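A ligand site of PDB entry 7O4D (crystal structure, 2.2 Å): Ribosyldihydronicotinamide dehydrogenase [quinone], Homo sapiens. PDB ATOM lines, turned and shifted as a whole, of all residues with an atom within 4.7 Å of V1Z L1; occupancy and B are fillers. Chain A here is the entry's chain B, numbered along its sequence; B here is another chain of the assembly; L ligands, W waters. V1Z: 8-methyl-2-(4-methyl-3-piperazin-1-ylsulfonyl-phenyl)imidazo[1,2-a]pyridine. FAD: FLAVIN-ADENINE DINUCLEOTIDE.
The side-chain amide oxygen of Asn 179 sits at hydrogen-bond distance from the side-chain hydroxyl of Tyr 150 of chain B, at 2.7 Å.
O of Met 172 lies within hydrogen-bond range of N of Asn 179.
O of Phe 196 of chain B is in hydrogen-bond range of N of Tyr 150 of chain B.
Residues that only touch V1Z L1: Trp 123 (3.7 Å), Phe 124 (3.8 Å), Gly 167 (3.1 Å), Met 172 (3.1 Å), Gln 140 of chain B (3.7 Å), Phe 144 of chain B (3.3 Å), Phe 149 of chain B (3.5 Å), Tyr 150 of chain B (3.9 Å) and Phe 196 of chain B (3.4 Å).
Hydrophobic or aromatic side chains that line V1Z L1: Trp 123, Phe 124, Met 172, Phe 144 of chain B, Phe 149 of chain B and Phe 196 of chain B.
Of the 16 residues printed, 11 come within 4 Å of V1Z L1.
N of Phe 124 sits at hydrogen-bond distance from O4 of FAD L2 (3.0 Å).
The backbone NH (N) of Gly 168 is in hydrogen-bond range of an oxygen (O2) of FAD L2.
N of Gly 168 sits at hydrogen-bond distance from O1 of V1Z L1 (3.0 Å).
The backbone NH of Gly 167 sits at hydrogen-bond distance from an oxygen (O2) of FAD L2 (3.0 Å).
The side-chain amide nitrogen of Asn 179 lies within hydrogen-bond range of an oxygen (O2) of V1Z L1 (3.1 Å).
The backbone NH (N) of Trp 123 is in hydrogen-bond range of a nitrogen (N5) of FAD L2.
An oxygen (O2) of FAD L2 is in hydrogen-bond range of the side-chain hydroxyl (OH) of Tyr 173.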
ATOM      1  N   TRP A 123      28.523  -0.447   6.576  1.00  0.00           N
ATOM      2  CA  TRP A 123      28.645   0.908   6.044  1.00  0.00           C
ATOM      3  C   TRP A 123      29.721   0.969   4.957  1.00  0.00           C
ATOM      4  O   TRP A 123      30.680   1.750   5.012  1.00  0.00           O
ATOM      5  CB  TRP A 123      28.940   1.914   7.164  1.00  0.00           C
ATOM      6  CG  TRP A 123      27.774   2.131   8.110  1.00  0.00           C
ATOM      7  CD1 TRP A 123      27.777   1.976   9.474  1.00  0.00           C
ATOM      8  CD2 TRP A 123      26.439   2.549   7.762  1.00  0.00           C
ATOM      9  NE1 TRP A 123      26.528   2.271   9.993  1.00  0.00           N
ATOM     10  CE2 TRP A 123      25.695   2.632   8.970  1.00  0.00           C
ATOM     11  CE3 TRP A 123      25.817   2.868   6.553  1.00  0.00           C
ATOM     12  CZ2 TRP A 123      24.342   3.014   8.985  1.00  0.00           C
ATOM     13  CZ3 TRP A 123      24.476   3.254   6.574  1.00  0.00           C
ATOM     14  CH2 TRP A 123      23.751   3.321   7.784  1.00  0.00           C
ATOM     15  N   PHE A 124      29.556   0.099   3.966  1.00  0.00           N
ATOM     16  CA  PHE A 124      30.440   0.024   2.799  1.00  0.00           C
ATOM     17  C   PHE A 124      31.880  -0.280   3.186  1.00  0.00           C
ATOM     18  O   PHE A 124      32.804   0.029   2.425  1.00  0.00           O
ATOM     19  CB  PHE A 124      30.370   1.301   1.951  1.00  0.00           C
ATOM     20  CG  PHE A 124      29.175   1.364   1.038  1.00  0.00           C
ATOM     21  CD1 PHE A 124      27.924   0.901   1.469  1.00  0.00           C
ATOM     22  CD2 PHE A 124      29.293   1.869  -0.258  1.00  0.00           C
ATOM     23  CE1 PHE A 124      26.813   0.967   0.629  1.00  0.00           C
ATOM     24  CE2 PHE A 124      28.179   1.945  -1.095  1.00  0.00           C
ATOM     25  CZ  PHE A 124      26.947   1.475  -0.651  1.00  0.00           C
ATOM     26  N   GLY A 167      24.233  -6.987   3.018  1.00  0.00           N
ATOM     27  CA  GLY A 167      22.787  -6.925   3.128  1.00  0.00           C
ATOM     28  C   GLY A 167      22.136  -6.798   1.757  1.00  0.00           C
ATOM     29  O   GLY A 167      21.087  -7.401   1.512  1.00  0.00           O
ATOM     30  N   GLY A 168      22.761  -6.047   0.853  1.00  0.00           N
ATOM     31  CA  GLY A 168      22.150  -5.794  -0.430  1.00  0.00           C
ATOM     32  C   GLY A 168      22.408  -6.914  -1.436  1.00  0.00           C
ATOM     33  O   GLY A 168      23.359  -7.684  -1.331  1.00  0.00           O
ATOM     34  N   MET A 172      21.671  -4.888  -6.728  1.00  0.00           N
ATOM     35  CA  MET A 172      21.786  -3.543  -6.153  1.00  0.00           C
ATOM     36  C   MET A 172      23.210  -3.019  -6.218  1.00  0.00           C
ATOM     37  O   MET A 172      23.419  -1.811  -6.297  1.00  0.00           O
ATOM     38  CB  MET A 172      21.263  -3.528  -4.714  1.00  0.00           C
ATOM     39  CG  MET A 172      19.763  -3.747  -4.632  1.00  0.00           C
ATOM     40  SD  MET A 172      19.243  -4.370  -3.016  1.00  0.00           S
ATOM     41  CE  MET A 172      20.304  -3.372  -2.039  1.00  0.00           C
ATOM     42  N   TYR A 173      24.197  -3.917  -6.222  1.00  0.00           N
ATOM     43  CA  TYR A 173      25.596  -3.507  -6.295  1.00  0.00           C
ATOM     44  C   TYR A 173      26.126  -3.617  -7.731  1.00  0.00           C
ATOM     45  O   TYR A 173      27.132  -4.292  -8.010  1.00  0.00           O
ATOM     46  CB  TYR A 173      26.443  -4.344  -5.339  1.00  0.00           C
ATOM     47  CG  TYR A 173      26.343  -3.882  -3.896  1.00  0.00           C
ATOM     48  CD1 TYR A 173      26.970  -2.709  -3.466  1.00  0.00           C
ATOM     49  CD2 TYR A 173      25.620  -4.629  -2.973  1.00  0.00           C
ATOM     50  CE1 TYR A 173      26.869  -2.290  -2.133  1.00  0.00           C
ATOM     51  CE2 TYR A 173      25.515  -4.209  -1.649  1.00  0.00           C
ATOM     52  CZ  TYR A 173      26.138  -3.044  -1.239  1.00  0.00           C
ATOM     53  OH  TYR A 173      26.051  -2.658   0.064  1.00  0.00           O
ATOM     54  N   ASN A 179      23.351   1.279  -5.185  1.00  0.00           N
ATOM     55  CA  ASN A 179      24.546   1.230  -4.347  1.00  0.00           C
ATOM     56  C   ASN A 179      25.843   1.403  -5.128  1.00  0.00           C
ATOM     57  O   ASN A 179      26.914   1.412  -4.516  1.00  0.00           O
ATOM     58  CB  ASN A 179      24.585  -0.091  -3.597  1.00  0.00           C
ATOM     59  CG  ASN A 179      23.445  -0.246  -2.631  1.00  0.00           C
ATOM     60  OD1 ASN A 179      22.749   0.724  -2.330  1.00  0.00           O
ATOM     61  ND2 ASN A 179      23.253  -1.450  -2.115  1.00  0.00           N
ATOM     62  N   GLY B  86      21.954  -6.631  14.062  1.00  0.00           N
ATOM     63  CA  GLY B  86      21.067  -5.709  13.366  1.00  0.00           C
ATOM     64  C   GLY B  86      19.628  -5.794  13.843  1.00  0.00           C
ATOM     65  O   GLY B  86      18.969  -4.772  14.055  1.00  0.00           O
ATOM     66  N   LEU B 138      24.186   4.912  14.217  1.00  0.00           N
ATOM     67  CA  LEU B 138      23.287   5.038  13.067  1.00  0.00           C
ATOM     68  C   LEU B 138      22.479   3.759  12.857  1.00  0.00           C
ATOM     69  O   LEU B 138      22.583   3.096  11.833  1.00  0.00           O
ATOM     70  CB  LEU B 138      24.095   5.404  11.827  1.00  0.00           C
ATOM     71  CG  LEU B 138      24.903   6.699  11.963  1.00  0.00           C
ATOM     72  CD1 LEU B 138      25.762   6.960  10.739  1.00  0.00           C
ATOM     73  CD2 LEU B 138      23.998   7.890  12.200  1.00  0.00           C
ATOM     74  N   GLN B 140      19.202   0.969  12.777  1.00  0.00           N
ATOM     75  CA  GLN B 140      17.938   0.860  12.066  1.00  0.00           C
ATOM     76  C   GLN B 140      16.801   1.408  12.911  1.00  0.00           C
ATOM     77  O   GLN B 140      16.719   1.148  14.120  1.00  0.00           O
ATOM     78  CB  GLN B 140      17.669  -0.612  11.698  1.00  0.00           C
ATOM     79  CG  GLN B 140      16.498  -0.758  10.741  1.00  0.00           C
ATOM     80  CD  GLN B 140      16.588  -2.020   9.892  1.00  0.00           C
ATOM     81  OE1 GLN B 140      17.453  -2.878  10.125  1.00  0.00           O
ATOM     82  NE2 GLN B 140      15.702  -2.127   8.907  1.00  0.00           N
ATOM     83  N   PHE B 144      17.729   5.064   9.481  1.00  0.00           N
ATOM     84  CA  PHE B 144      17.208   4.533   8.234  1.00  0.00           C
ATOM     85  C   PHE B 144      16.252   3.411   8.591  1.00  0.00           C
ATOM     86  O   PHE B 144      16.284   2.867   9.693  1.00  0.00           O
ATOM     87  CB  PHE B 144      18.321   4.011   7.324  1.00  0.00           C
ATOM     88  CG  PHE B 144      18.866   2.697   7.780  1.00  0.00           C
ATOM     89  CD1 PHE B 144      19.864   2.644   8.731  1.00  0.00           C
ATOM     90  CD2 PHE B 144      18.321   1.516   7.315  1.00  0.00           C
ATOM     91  CE1 PHE B 144      20.326   1.442   9.184  1.00  0.00           C
ATOM     92  CE2 PHE B 144      18.787   0.313   7.777  1.00  0.00           C
ATOM     93  CZ  PHE B 144      19.804   0.272   8.700  1.00  0.00           C
ATOM     94  N   ILE B 146      13.329   0.472   6.214  1.00  0.00           N
ATOM     95  CA  ILE B 146      12.591   0.228   4.987  1.00  0.00           C
ATOM     96  C   ILE B 146      11.232   0.901   5.151  1.00  0.00           C
ATOM     97  O   ILE B 146      10.505   0.568   6.101  1.00  0.00           O
ATOM     98  CB  ILE B 146      12.468  -1.274   4.698  1.00  0.00           C
ATOM     99  CG1 ILE B 146      13.875  -1.825   4.489  1.00  0.00           C
ATOM    100  CG2 ILE B 146      11.615  -1.528   3.431  1.00  0.00           C
ATOM    101  CD1 ILE B 146      13.992  -3.299   4.796  1.00  0.00           C
ATOM    102  N   PHE B 149      15.566   5.391   3.080  1.00  0.00           N
ATOM    103  CA  PHE B 149      17.014   5.357   2.886  1.00  0.00           C
ATOM    104  C   PHE B 149      17.355   6.175   1.647  1.00  0.00           C
ATOM    105  O   PHE B 149      16.498   6.427   0.801  1.00  0.00           O
ATOM    106  CB  PHE B 149      17.545   3.915   2.776  1.00  0.00           C
ATOM    107  CG  PHE B 149      16.909   3.101   1.668  1.00  0.00           C
ATOM    108  CD1 PHE B 149      15.739   2.381   1.909  1.00  0.00           C
ATOM    109  CD2 PHE B 149      17.510   3.020   0.420  1.00  0.00           C
ATOM    110  CE1 PHE B 149      15.154   1.609   0.891  1.00  0.00           C
ATOM    111  CE2 PHE B 149      16.939   2.265  -0.603  1.00  0.00           C
ATOM    112  CZ  PHE B 149      15.764   1.569  -0.380  1.00  0.00           C
ATOM    113  N   TYR B 150      18.637   6.548   1.556  1.00  0.00           N
ATOM    114  CA  TYR B 150      19.129   7.500   0.556  1.00  0.00           C
ATOM    115  C   TYR B 150      18.265   8.747   0.692  1.00  0.00           C
ATOM    116  O   TYR B 150      18.092   9.212   1.830  1.00  0.00           O
ATOM    117  CB  TYR B 150      19.162   6.842  -0.829  1.00  0.00           C
ATOM    118  CG  TYR B 150      20.305   5.868  -0.988  1.00  0.00           C
ATOM    119  CD1 TYR B 150      21.602   6.240  -0.620  1.00  0.00           C
ATOM    120  CD2 TYR B 150      20.105   4.598  -1.491  1.00  0.00           C
ATOM    121  CE1 TYR B 150      22.652   5.361  -0.768  1.00  0.00           C
ATOM    122  CE2 TYR B 150      21.147   3.715  -1.635  1.00  0.00           C
ATOM    123  CZ  TYR B 150      22.416   4.099  -1.267  1.00  0.00           C
ATOM    124  OH  TYR B 150      23.446   3.213  -1.417  1.00  0.00           O
ATOM    125  N   GLY B 192      27.639   5.752   0.891  1.00  0.00           N
ATOM    126  CA  GLY B 192      27.186   4.537   1.556  1.00  0.00           C
ATOM    127  C   GLY B 192      26.718   4.767   2.985  1.00  0.00           C
ATOM    128  O   GLY B 192      25.913   3.995   3.518  1.00  0.00           O
ATOM    129  N   PHE B 196      23.078   7.573   2.610  1.00  0.00           N
ATOM    130  CA  PHE B 196      22.153   6.465   2.793  1.00  0.00           C
ATOM    131  C   PHE B 196      21.155   6.760   3.902  1.00  0.00           C
ATOM    132  O   PHE B 196      19.999   6.323   3.831  1.00  0.00           O
ATOM    133  CB  PHE B 196      22.901   5.172   3.113  1.00  0.00           C
ATOM    134  CG  PHE B 196      21.999   3.980   3.325  1.00  0.00           C
ATOM    135  CD1 PHE B 196      21.527   3.248   2.251  1.00  0.00           C
ATOM    136  CD2 PHE B 196      21.616   3.602   4.606  1.00  0.00           C
ATOM    137  CE1 PHE B 196      20.701   2.143   2.426  1.00  0.00           C
ATOM    138  CE2 PHE B 196      20.761   2.504   4.804  1.00  0.00           C
ATOM    139  CZ  PHE B 196      20.306   1.774   3.692  1.00  0.00           C
HETATM  140  C   V1Z L   1      21.610  -2.882   9.492  1.00  0.00           C
HETATM  141  C4  V1Z L   1      22.158  -2.052   8.386  1.00  0.00           C
HETATM  142  N2  V1Z L   1      22.057  -2.170   7.035  1.00  0.00           N
HETATM  143  C5  V1Z L   1      22.765  -1.159   6.481  1.00  0.00           C
HETATM  144  C7  V1Z L   1      22.214  -1.726   4.129  1.00  0.00           C
HETATM  145  C8  V1Z L   1      22.262  -1.518   2.747  1.00  0.00           C
HETATM  146  C3  V1Z L   1      23.110   0.025   0.803  1.00  0.00           C
HETATM  147  C2  V1Z L   1      23.155  -0.613   9.947  1.00  0.00           C
HETATM  148  C9  V1Z L   1      20.780  -4.118   9.184  1.00  0.00           C
HETATM  149  C10 V1Z L   1      21.891  -2.507  10.784  1.00  0.00           C
HETATM  150  C11 V1Z L   1      23.263  -0.388   7.513  1.00  0.00           C
HETATM  151  C12 V1Z L   1      23.015  -0.324   2.271  1.00  0.00           C
HETATM  152  C1  V1Z L   1      22.660  -1.372  11.003  1.00  0.00           C
HETATM  153  N1  V1Z L   1      22.904  -0.960   8.676  1.00  0.00           N
HETATM  154  C13 V1Z L   1      23.653   0.493   3.206  1.00  0.00           C
HETATM  155  C14 V1Z L   1      23.571   0.235   4.566  1.00  0.00           C
HETATM  156  C15 V1Z L   1      19.051  -2.513   2.737  1.00  0.00           C
HETATM  157  C16 V1Z L   1      22.880  -0.880   5.021  1.00  0.00           C
HETATM  158  C17 V1Z L   1      17.887  -1.552   2.979  1.00  0.00           C
HETATM  159  C19 V1Z L   1      17.981  -0.891   0.654  1.00  0.00           C
HETATM  160  C20 V1Z L   1      19.306  -1.655   0.508  1.00  0.00           C
HETATM  161  N18 V1Z L   1      17.134  -1.438   1.715  1.00  0.00           N
HETATM  162  N9  V1Z L   1      19.970  -1.827   1.806  1.00  0.00           N
HETATM  163  O1  V1Z L   1      21.324  -3.848   2.396  1.00  0.00           O
HETATM  164  O2  V1Z L   1      22.010  -2.626   0.489  1.00  0.00           O
HETATM  165  S1  V1Z L   1      21.448  -2.541   1.785  1.00  0.00           S
HETATM  166  PA  FAD L   2      23.115 -14.160   9.108  1.00  0.00           P
HETATM  167  O1A FAD L   2      21.816 -13.537   9.408  1.00  0.00           O
HETATM  168  O2A FAD L   2      23.900 -14.724  10.203  1.00  0.00           O
HETATM  169  O5B FAD L   2      22.828 -15.306   7.945  1.00  0.00           O
HETATM  170  C5B FAD L   2      21.556 -15.195   7.304  1.00  0.00           C
HETATM  171  C4B FAD L   2      20.611 -16.433   7.293  1.00  0.00           C
HETATM  172  O4B FAD L   2      21.916 -17.195   7.427  1.00  0.00           O
HETATM  173  C3B FAD L   2      20.073 -17.363   8.378  1.00  0.00           C
HETATM  174  O3B FAD L   2      19.205 -18.356   7.819  1.00  0.00           O
HETATM  175  C2B FAD L   2      21.271 -17.996   8.974  1.00  0.00           C
HETATM  176  O2B FAD L   2      20.930 -19.012   9.908  1.00  0.00           O
HETATM  177  C1B FAD L   2      21.659 -18.601   7.556  1.00  0.00           C
HETATM  178  N9A FAD L   2      22.914 -19.411   7.685  1.00  0.00           N
HETATM  179  C8A FAD L   2      23.959 -19.444   8.511  1.00  0.00           C
HETATM  180  N7A FAD L   2      24.737 -20.480   8.141  1.00  0.00           N
HETATM  181  C5A FAD L   2      24.179 -21.110   7.108  1.00  0.00           C
HETATM  182  C6A FAD L   2      24.511 -22.193   6.366  1.00  0.00           C
HETATM  183  N6A FAD L   2      25.650 -22.814   6.641  1.00  0.00           N
HETATM  184  N1A FAD L   2      23.761 -22.646   5.358  1.00  0.00           N
HETATM  185  C2A FAD L   2      22.578 -21.984   5.071  1.00  0.00           C
HETATM  186  N3A FAD L   2      22.243 -20.879   5.859  1.00  0.00           N
HETATM  187  C4A FAD L   2      23.029 -20.465   6.861  1.00  0.00           C
HETATM  188  N1  FAD L   2      24.773  -4.299   4.224  1.00  0.00           N
HETATM  189  C2  FAD L   2      25.090  -3.717   2.993  1.00  0.00           C
HETATM  190  O2  FAD L   2      24.797  -4.261   1.933  1.00  0.00           O
HETATM  191  N3  FAD L   2      25.764  -2.491   2.974  1.00  0.00           N
HETATM  192  C4  FAD L   2      26.106  -1.873   4.180  1.00  0.00           C
HETATM  193  O4  FAD L   2      26.702  -0.810   4.140  1.00  0.00           O
HETATM  194  C4X FAD L   2      25.767  -2.471   5.398  1.00  0.00           C
HETATM  195  N5  FAD L   2      26.100  -1.865   6.597  1.00  0.00           N
HETATM  196  C5X FAD L   2      25.770  -2.500   7.798  1.00  0.00           C
HETATM  197  C6  FAD L   2      26.095  -1.889   9.011  1.00  0.00           C
HETATM  198  C7  FAD L   2      25.765  -2.492  10.215  1.00  0.00           C
HETATM  199  C7M FAD L   2      26.133  -1.827  11.392  1.00  0.00           C
HETATM  200  C8  FAD L   2      25.078  -3.730  10.217  1.00  0.00           C
HETATM  201  C8M FAD L   2      24.711  -4.405  11.398  1.00  0.00           C
HETATM  202  C9  FAD L   2      24.748  -4.308   8.997  1.00  0.00           C
HETATM  203  C9A FAD L   2      25.087  -3.710   7.779  1.00  0.00           C
HETATM  204  N10 FAD L   2      24.773  -4.291   6.595  1.00  0.00           N
HETATM  205  C10 FAD L   2      25.106  -3.693   5.423  1.00  0.00           C
HETATM  206  C1' FAD L   2      24.083  -5.613   6.528  1.00  0.00           C
HETATM  207  C2' FAD L   2      25.122  -6.749   6.727  1.00  0.00           C
HETATM  208  O2' FAD L   2      26.222  -6.640   5.817  1.00  0.00           O
HETATM  209  C3' FAD L   2      24.443  -8.134   6.619  1.00  0.00           C
HETATM  210  O3' FAD L   2      23.377  -8.216   7.560  1.00  0.00           O
HETATM  211  C4' FAD L   2      25.453  -9.263   6.841  1.00  0.00           C
HETATM  212  O4' FAD L   2      26.400  -9.216   5.763  1.00  0.00           O
HETATM  213  C5' FAD L   2      24.708 -10.606   6.785  1.00  0.00           C
HETATM  214  O5' FAD L   2      25.482 -11.818   7.022  1.00  0.00           O
HETATM  215  P   FAD L   2      25.439 -12.465   8.506  1.00  0.00           P
HETATM  216  O1P FAD L   2      26.390 -13.599   8.600  1.00  0.00           O
HETATM  217  O2P FAD L   2      25.471 -11.430   9.572  1.00  0.00           O
HETATM  218  O3P FAD L   2      23.884 -12.925   8.510  1.00  0.00           O
HETATM  219  O   HOH W   1      20.621  -1.526  13.854  1.00  0.00           O
